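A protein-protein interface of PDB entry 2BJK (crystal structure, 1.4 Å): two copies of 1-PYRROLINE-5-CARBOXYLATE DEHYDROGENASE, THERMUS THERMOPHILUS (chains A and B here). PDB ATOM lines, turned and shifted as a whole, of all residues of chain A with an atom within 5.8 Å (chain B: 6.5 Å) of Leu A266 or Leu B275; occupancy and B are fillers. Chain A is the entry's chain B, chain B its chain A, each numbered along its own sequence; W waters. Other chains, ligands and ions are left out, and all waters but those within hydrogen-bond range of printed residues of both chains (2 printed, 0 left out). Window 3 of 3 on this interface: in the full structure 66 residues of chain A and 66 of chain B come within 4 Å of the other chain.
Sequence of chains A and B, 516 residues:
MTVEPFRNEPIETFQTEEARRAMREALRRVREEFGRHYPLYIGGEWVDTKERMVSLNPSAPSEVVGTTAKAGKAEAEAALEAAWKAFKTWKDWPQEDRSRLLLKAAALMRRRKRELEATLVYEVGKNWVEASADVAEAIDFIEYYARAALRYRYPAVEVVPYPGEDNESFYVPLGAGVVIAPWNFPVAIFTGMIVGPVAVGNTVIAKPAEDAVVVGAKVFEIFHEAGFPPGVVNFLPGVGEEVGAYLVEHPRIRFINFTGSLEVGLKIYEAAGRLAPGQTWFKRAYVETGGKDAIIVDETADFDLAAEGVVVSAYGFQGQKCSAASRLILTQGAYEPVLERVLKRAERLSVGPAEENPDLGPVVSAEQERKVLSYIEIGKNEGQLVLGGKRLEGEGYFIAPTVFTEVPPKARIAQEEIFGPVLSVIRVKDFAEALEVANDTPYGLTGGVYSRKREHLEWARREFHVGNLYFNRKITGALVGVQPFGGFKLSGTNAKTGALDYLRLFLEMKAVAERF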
ATOM      1  N   SER A 261     -37.505 -15.131  -7.450  1.00  0.00           N
ATOM      2  CA  SER A 261     -36.879 -16.032  -8.412  1.00  0.00           C
ATOM      3  C   SER A 261     -35.756 -15.388  -9.209  1.00  0.00           C
ATOM      4  O   SER A 261     -35.709 -14.171  -9.381  1.00  0.00           O
ATOM      5  CB  SER A 261     -37.925 -16.562  -9.393  1.00  0.00           C
ATOM      6  OG  SER A 261     -38.383 -15.526 -10.242  1.00  0.00           O
ATOM      7  N   LEU A 262     -34.855 -16.223  -9.708  1.00  0.00           N
ATOM      8  CA  LEU A 262     -33.754 -15.731 -10.513  1.00  0.00           C
ATOM      9  C   LEU A 262     -34.299 -15.125 -11.804  1.00  0.00           C
ATOM     10  O   LEU A 262     -33.835 -14.079 -12.252  1.00  0.00           O
ATOM     11  CB  LEU A 262     -32.788 -16.871 -10.837  1.00  0.00           C
ATOM     12  CG  LEU A 262     -31.679 -16.517 -11.827  1.00  0.00           C
ATOM     13  CD1 LEU A 262     -30.850 -15.345 -11.301  1.00  0.00           C
ATOM     14  CD2 LEU A 262     -30.807 -17.742 -12.049  1.00  0.00           C
ATOM     15  N   GLU A 263     -35.294 -15.782 -12.393  1.00  0.00           N
ATOM     16  CA  GLU A 263     -35.894 -15.303 -13.631  1.00  0.00           C
ATOM     17  C   GLU A 263     -36.308 -13.842 -13.509  1.00  0.00           C
ATOM     18  O   GLU A 263     -35.964 -13.011 -14.350  1.00  0.00           O
ATOM     19  CB  GLU A 263     -37.115 -16.158 -13.985  1.00  0.00           C
ATOM     20  CG  GLU A 263     -37.853 -15.710 -15.234  1.00  0.00           C
ATOM     21  CD  GLU A 263     -39.117 -16.512 -15.476  1.00  0.00           C
ATOM     22  OE1 GLU A 263     -39.017 -17.745 -15.652  1.00  0.00           O
ATOM     23  OE2 GLU A 263     -40.212 -15.910 -15.485  1.00  0.00           O
ATOM     24  N   VAL A 264     -37.042 -13.529 -12.448  1.00  0.00           N
ATOM     25  CA  VAL A 264     -37.500 -12.167 -12.230  1.00  0.00           C
ATOM     26  C   VAL A 264     -36.351 -11.255 -11.790  1.00  0.00           C
ATOM     27  O   VAL A 264     -36.261 -10.104 -12.221  1.00  0.00           O
ATOM     28  CB  VAL A 264     -38.638 -12.145 -11.189  1.00  0.00           C
ATOM     29  CG1 VAL A 264     -39.018 -10.717 -10.854  1.00  0.00           C
ATOM     30  CG2 VAL A 264     -39.848 -12.907 -11.746  1.00  0.00           C
ATOM     31  N   GLY A 265     -35.467 -11.778 -10.944  1.00  0.00           N
ATOM     32  CA  GLY A 265     -34.338 -10.989 -10.481  1.00  0.00           C
ATOM     33  C   GLY A 265     -33.455 -10.496 -11.615  1.00  0.00           C
ATOM     34  O   GLY A 265     -32.942  -9.373 -11.574  1.00  0.00           O
ATOM     35  N   LEU A 266     -33.268 -11.334 -12.630  1.00  0.00           N
ATOM     36  CA  LEU A 266     -32.450 -10.959 -13.777  1.00  0.00           C
ATOM     37  C   LEU A 266     -33.082  -9.789 -14.523  1.00  0.00           C
ATOM     38  O   LEU A 266     -32.392  -8.857 -14.924  1.00  0.00           O
ATOM     39  CB  LEU A 266     -32.278 -12.149 -14.724  1.00  0.00           C
ATOM     40  CG  LEU A 266     -31.349 -13.261 -14.231  1.00  0.00           C
ATOM     41  CD1 LEU A 266     -31.433 -14.454 -15.173  1.00  0.00           C
ATOM     42  CD2 LEU A 266     -29.912 -12.740 -14.145  1.00  0.00           C
ATOM     43  N   LYS A 267     -34.400  -9.837 -14.701  1.00  0.00           N
ATOM     44  CA  LYS A 267     -35.108  -8.769 -15.397  1.00  0.00           C
ATOM     45  C   LYS A 267     -35.032  -7.464 -14.615  1.00  0.00           C
ATOM     46  O   LYS A 267     -34.852  -6.388 -15.189  1.00  0.00           O
ATOM     47  CB  LYS A 267     -36.574  -9.154 -15.603  1.00  0.00           C
ATOM     48  CG  LYS A 267     -36.782 -10.326 -16.546  1.00  0.00           C
ATOM     49  CD  LYS A 267     -38.259 -10.663 -16.692  1.00  0.00           C
ATOM     50  CE  LYS A 267     -38.467 -11.825 -17.647  1.00  0.00           C
ATOM     51  NZ  LYS A 267     -39.909 -12.159 -17.796  1.00  0.00           N
ATOM     52  N   ILE A 268     -35.174  -7.561 -13.299  1.00  0.00           N
ATOM     53  CA  ILE A 268     -35.127  -6.379 -12.456  1.00  0.00           C
ATOM     54  C   ILE A 268     -33.742  -5.743 -12.468  1.00  0.00           C
ATOM     55  O   ILE A 268     -33.615  -4.529 -12.606  1.00  0.00           O
ATOM     56  CB  ILE A 268     -35.544  -6.724 -11.009  1.00  0.00           C
ATOM     57  CG1 ILE A 268     -37.042  -7.042 -10.976  1.00  0.00           C
ATOM     58  CG2 ILE A 268     -35.209  -5.573 -10.069  1.00  0.00           C
ATOM     59  CD1 ILE A 268     -37.564  -7.432  -9.614  1.00  0.00           C
ATOM     60  N   TYR A 269     -32.703  -6.561 -12.348  1.00  0.00           N
ATOM     61  CA  TYR A 269     -31.344  -6.030 -12.342  1.00  0.00           C
ATOM     62  C   TYR A 269     -31.031  -5.354 -13.672  1.00  0.00           C
ATOM     63  O   TYR A 269     -30.372  -4.316 -13.710  1.00  0.00           O
ATOM     64  CB  TYR A 269     -30.337  -7.145 -12.081  1.00  0.00           C
ATOM     65  CG  TYR A 269     -29.015  -6.655 -11.529  1.00  0.00           C
ATOM     66  CD1 TYR A 269     -27.835  -6.782 -12.264  1.00  0.00           C
ATOM     67  CD2 TYR A 269     -28.943  -6.101 -10.252  1.00  0.00           C
ATOM     68  CE1 TYR A 269     -26.611  -6.372 -11.733  1.00  0.00           C
ATOM     69  CE2 TYR A 269     -27.729  -5.687  -9.715  1.00  0.00           C
ATOM     70  CZ  TYR A 269     -26.568  -5.830 -10.459  1.00  0.00           C
ATOM     71  OH  TYR A 269     -25.364  -5.451  -9.912  1.00  0.00           O
ATOM     72  N   GLU A 270     -31.506  -5.943 -14.765  1.00  0.00           N
ATOM     73  CA  GLU A 270     -31.263  -5.368 -16.080  1.00  0.00           C
ATOM     74  C   GLU A 270     -31.996  -4.033 -16.217  1.00  0.00           C
ATOM     75  O   GLU A 270     -31.425  -3.046 -16.683  1.00  0.00           O
ATOM     76  CB  GLU A 270     -31.723  -6.339 -17.172  1.00  0.00           C
ATOM     77  CG  GLU A 270     -31.363  -5.894 -18.580  1.00  0.00           C
ATOM     78  CD  GLU A 270     -31.785  -6.898 -19.635  1.00  0.00           C
ATOM     79  OE1 GLU A 270     -31.422  -8.084 -19.505  1.00  0.00           O
ATOM     80  OE2 GLU A 270     -32.477  -6.497 -20.596  1.00  0.00           O
ATOM     81  N   ALA A 271     -33.259  -3.999 -15.804  1.00  0.00           N
ATOM     82  CA  ALA A 271     -34.046  -2.773 -15.887  1.00  0.00           C
ATOM     83  C   ALA A 271     -33.451  -1.664 -15.019  1.00  0.00           C
ATOM     84  O   ALA A 271     -33.436  -0.498 -15.416  1.00  0.00           O
ATOM     85  CB  ALA A 271     -35.491  -3.045 -15.468  1.00  0.00           C
ATOM     86  N   THR A 289     -31.880 -13.921  -5.051  1.00  0.00           N
ATOM     87  CA  THR A 289     -32.586 -14.901  -5.835  1.00  0.00           C
ATOM     88  C   THR A 289     -32.539 -16.309  -5.252  1.00  0.00           C
ATOM     89  O   THR A 289     -32.280 -16.486  -4.062  1.00  0.00           O
ATOM     90  CB  THR A 289     -32.042 -14.838  -7.266  1.00  0.00           C
ATOM     91  OG1 THR A 289     -30.624 -14.618  -7.220  1.00  0.00           O
ATOM     92  CG2 THR A 289     -32.670 -13.665  -8.012  1.00  0.00           C
ATOM     93  N   LEU A 490     -25.400 -16.515  -8.964  1.00  0.00           N
ATOM     94  CA  LEU A 490     -26.766 -16.172  -9.335  1.00  0.00           C
ATOM     95  C   LEU A 490     -27.789 -16.285  -8.216  1.00  0.00           C
ATOM     96  O   LEU A 490     -28.998 -16.286  -8.456  1.00  0.00           O
ATOM     97  CB  LEU A 490     -27.204 -16.946 -10.586  1.00  0.00           C
ATOM     98  CG  LEU A 490     -26.411 -16.517 -11.834  1.00  0.00           C
ATOM     99  CD1 LEU A 490     -26.995 -17.181 -13.072  1.00  0.00           C
ATOM    100  CD2 LEU A 490     -26.441 -15.003 -11.992  1.00  0.00           C
ATOM    101  N   ALA B 271     -24.893  -1.960 -19.445  1.00  0.00           N
ATOM    102  CA  ALA B 271     -24.301  -3.227 -19.854  1.00  0.00           C
ATOM    103  C   ALA B 271     -24.034  -4.135 -18.656  1.00  0.00           C
ATOM    104  O   ALA B 271     -24.221  -5.347 -18.736  1.00  0.00           O
ATOM    105  CB  ALA B 271     -23.004  -2.977 -20.621  1.00  0.00           C
ATOM    106  N   ALA B 272     -23.605  -3.550 -17.541  1.00  0.00           N
ATOM    107  CA  ALA B 272     -23.313  -4.327 -16.338  1.00  0.00           C
ATOM    108  C   ALA B 272     -24.562  -4.996 -15.777  1.00  0.00           C
ATOM    109  O   ALA B 272     -24.472  -6.010 -15.082  1.00  0.00           O
ATOM    110  CB  ALA B 272     -22.683  -3.432 -15.272  1.00  0.00           C
ATOM    111  N   GLY B 273     -25.723  -4.426 -16.076  1.00  0.00           N
ATOM    112  CA  GLY B 273     -26.967  -4.992 -15.583  1.00  0.00           C
ATOM    113  C   GLY B 273     -27.456  -6.191 -16.372  1.00  0.00           C
ATOM    114  O   GLY B 273     -28.380  -6.879 -15.943  1.00  0.00           O
ATOM    115  N   ARG B 274     -26.829  -6.447 -17.516  1.00  0.00           N
ATOM    116  CA  ARG B 274     -27.211  -7.565 -18.377  1.00  0.00           C
ATOM    117  C   ARG B 274     -26.438  -8.837 -18.044  1.00  0.00           C
ATOM    118  O   ARG B 274     -25.276  -8.786 -17.634  1.00  0.00           O
ATOM    119  CB  ARG B 274     -26.953  -7.216 -19.852  1.00  0.00           C
ATOM    120  CG  ARG B 274     -27.653  -5.961 -20.360  1.00  0.00           C
ATOM    121  CD  ARG B 274     -27.616  -5.882 -21.889  1.00  0.00           C
ATOM    122  NE  ARG B 274     -26.263  -5.756 -22.433  1.00  0.00           N
ATOM    123  CZ  ARG B 274     -25.710  -4.610 -22.825  1.00  0.00           C
ATOM    124  NH1 ARG B 274     -24.473  -4.600 -23.303  1.00  0.00           N
ATOM    125  NH2 ARG B 274     -26.394  -3.477 -22.750  1.00  0.00           N
ATOM    126  N   LEU B 275     -27.087  -9.984 -18.217  1.00  0.00           N
ATOM    127  CA  LEU B 275     -26.432 -11.260 -17.982  1.00  0.00           C
ATOM    128  C   LEU B 275     -25.884 -11.731 -19.330  1.00  0.00           C
ATOM    129  O   LEU B 275     -26.640 -12.191 -20.191  1.00  0.00           O
ATOM    130  CB  LEU B 275     -27.425 -12.300 -17.450  1.00  0.00           C
ATOM    131  CG  LEU B 275     -26.796 -13.626 -17.007  1.00  0.00           C
ATOM    132  CD1 LEU B 275     -26.106 -13.449 -15.656  1.00  0.00           C
ATOM    133  CD2 LEU B 275     -27.873 -14.702 -16.911  1.00  0.00           C
ATOM    134  N   ALA B 276     -24.580 -11.590 -19.527  1.00  0.00           N
ATOM    135  CA  ALA B 276     -23.967 -12.028 -20.775  1.00  0.00           C
ATOM    136  C   ALA B 276     -24.099 -13.546 -20.857  1.00  0.00           C
ATOM    137  O   ALA B 276     -24.215 -14.223 -19.833  1.00  0.00           O
ATOM    138  CB  ALA B 276     -22.501 -11.622 -20.810  1.00  0.00           C
ATOM    139  N   PRO B 277     -24.094 -14.105 -22.077  1.00  0.00           N
ATOM    140  CA  PRO B 277     -24.218 -15.557 -22.225  1.00  0.00           C
ATOM    141  C   PRO B 277     -23.178 -16.327 -21.414  1.00  0.00           C
ATOM    142  O   PRO B 277     -21.974 -16.125 -21.583  1.00  0.00           O
ATOM    143  CB  PRO B 277     -24.048 -15.761 -23.729  1.00  0.00           C
ATOM    144  CG  PRO B 277     -24.659 -14.520 -24.293  1.00  0.00           C
ATOM    145  CD  PRO B 277     -24.091 -13.442 -23.393  1.00  0.00           C
ATOM    146  N   GLY B 278     -23.652 -17.201 -20.530  1.00  0.00           N
ATOM    147  CA  GLY B 278     -22.757 -17.999 -19.711  1.00  0.00           C
ATOM    148  C   GLY B 278     -22.308 -17.349 -18.411  1.00  0.00           C
ATOM    149  O   GLY B 278     -21.607 -17.972 -17.616  1.00  0.00           O
ATOM    150  N   GLN B 279     -22.711 -16.102 -18.195  1.00  0.00           N
ATOM    151  CA  GLN B 279     -22.339 -15.365 -16.988  1.00  0.00           C
ATOM    152  C   GLN B 279     -22.990 -16.008 -15.760  1.00  0.00           C
ATOM    153  O   GLN B 279     -24.160 -16.382 -15.795  1.00  0.00           O
ATOM    154  CB  GLN B 279     -22.788 -13.915 -17.140  1.00  0.00           C
ATOM    155  CG  GLN B 279     -22.256 -12.952 -16.102  1.00  0.00           C
ATOM    156  CD  GLN B 279     -22.674 -11.536 -16.419  1.00  0.00           C
ATOM    157  OE1 GLN B 279     -22.439 -11.049 -17.528  1.00  0.00           O
ATOM    158  NE2 GLN B 279     -23.297 -10.866 -15.457  1.00  0.00           N
ATOM    159  N   THR B 280     -22.232 -16.125 -14.673  1.00  0.00           N
ATOM    160  CA  THR B 280     -22.744 -16.757 -13.460  1.00  0.00           C
ATOM    161  C   THR B 280     -22.774 -15.872 -12.214  1.00  0.00           C
ATOM    162  O   THR B 280     -22.628 -16.358 -11.090  1.00  0.00           O
ATOM    163  CB  THR B 280     -21.942 -18.029 -13.134  1.00  0.00           C
ATOM    164  OG1 THR B 280     -20.551 -17.703 -13.052  1.00  0.00           O
ATOM    165  CG2 THR B 280     -22.154 -19.084 -14.215  1.00  0.00           C
ATOM    166  N   TRP B 281     -22.969 -14.576 -12.411  1.00  0.00           N
ATOM    167  CA  TRP B 281     -23.054 -13.644 -11.291  1.00  0.00           C
ATOM    168  C   TRP B 281     -23.683 -12.348 -11.737  1.00  0.00           C
ATOM    169  O   TRP B 281     -23.871 -12.115 -12.931  1.00  0.00           O
ATOM    170  CB  TRP B 281     -21.662 -13.347 -10.710  1.00  0.00           C
ATOM    171  CG  TRP B 281     -20.641 -12.897 -11.728  1.00  0.00           C
ATOM    172  CD1 TRP B 281     -20.672 -11.760 -12.493  1.00  0.00           C
ATOM    173  CD2 TRP B 281     -19.438 -13.583 -12.082  1.00  0.00           C
ATOM    174  NE1 TRP B 281     -19.559 -11.702 -13.301  1.00  0.00           N
ATOM    175  CE2 TRP B 281     -18.785 -12.808 -13.068  1.00  0.00           C
ATOM    176  CE3 TRP B 281     -18.845 -14.780 -11.660  1.00  0.00           C
ATOM    177  CZ2 TRP B 281     -17.565 -13.195 -13.638  1.00  0.00           C
ATOM    178  CZ3 TRP B 281     -17.634 -15.164 -12.228  1.00  0.00           C
ATOM    179  CH2 TRP B 281     -17.009 -14.372 -13.207  1.00  0.00           C
ATOM    180  N   PHE B 282     -24.035 -11.520 -10.761  1.00  0.00           N
ATOM    181  CA  PHE B 282     -24.580 -10.204 -11.038  1.00  0.00           C
ATOM    182  C   PHE B 282     -23.360  -9.291 -10.959  1.00  0.00           C
ATOM    183  O   PHE B 282     -22.740  -9.154  -9.902  1.00  0.00           O
ATOM    184  CB  PHE B 282     -25.612  -9.801  -9.982  1.00  0.00           C
ATOM    185  CG  PHE B 282     -26.908 -10.553 -10.083  1.00  0.00           C
ATOM    186  CD1 PHE B 282     -27.057 -11.798  -9.484  1.00  0.00           C
ATOM    187  CD2 PHE B 282     -27.976 -10.019 -10.796  1.00  0.00           C
ATOM    188  CE1 PHE B 282     -28.257 -12.505  -9.592  1.00  0.00           C
ATOM    189  CE2 PHE B 282     -29.177 -10.716 -10.910  1.00  0.00           C
ATOM    190  CZ  PHE B 282     -29.318 -11.962 -10.307  1.00  0.00           C
HETATM  191  O   HOH W   1     -30.018  -9.962 -18.095  1.00  0.00           O
HETATM  192  O   HOH W   2     -29.644  -9.166 -15.401  1.00  0.00           O
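The backbone NH (N) of Glu A270 sits close to the backbone carbonyl oxygen (O) of Gly B273 (3.5 Å).
The backbone carbonyl oxygen of Thr B280 lies within hydrogen-bond range of the backbone NH of Leu A490.
NE2 of Gln B279 lies within hydrogen-bond range of O of Trp B281, 2.9 Å away.
OG1 of Thr A289 lies within hydrogen-bond range of O of Leu A490, 2.6 Å away.
Phe B282 touches Leu A262.
Leu A266 touches Leu B275 (CD2 to CD2, 3.96 Å).
Leu A266 touches Phe B282 (CD2 to CE2, 3.9 Å).
CE1 of Tyr A269 touches O of Ala B272, at 3.99 Å.
Tyr A269 touches Gly B273.
Tyr A269 touches Phe B282 (CD1 to CD2, 3.6 Å).
OG1 of Thr A289 touches CE1 of Phe B282, 3.96 Å away.
Leu A490 touches Leu B275.
CD2 of Leu A490 touches N of Trp B281, at 3.5 Å.
CD2 of Leu A490 touches CE1 of Phe B282, 3.9 Å away.
Of chain B, only Leu B275 (3.96 Å) and Phe B282 (3.9 Å) come within 4 Å of Leu A266.
Of the printed residues of chain B, Leu A490 touches Leu B275, Thr B280, Trp B281 and Phe B282.
Printed residues of chain A within 4 Å of Leu B275: Leu A266 (3.96 Å) and Leu A490 (3.99 Å).
Of the printed residues of chain A, Trp B281 touches Leu A490.
The nearest residue of chain B that does not touch Leu A266 is Gly B273 (4.6 Å).
Of the 13 printed residues of chain A, 6 touch a printed residue of chain B.
Among the printed residues, no Asp or Glu carboxylate lies within 4 Å of a Lys or Arg side-chain nitrogen of the other chain.
1 position is printed for both chains.
Water W2 bridges the backbone carbonyl oxygen (O) of Gly B273 (2.7 Å) and the backbone carbonyl oxygen (O) of Leu A266 (2.8 Å).
Water W1 bridges the side-chain carboxylate (OE1) of Glu A270 (2.7 Å) and the backbone NH (N) of Leu B275 (2.9 Å).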
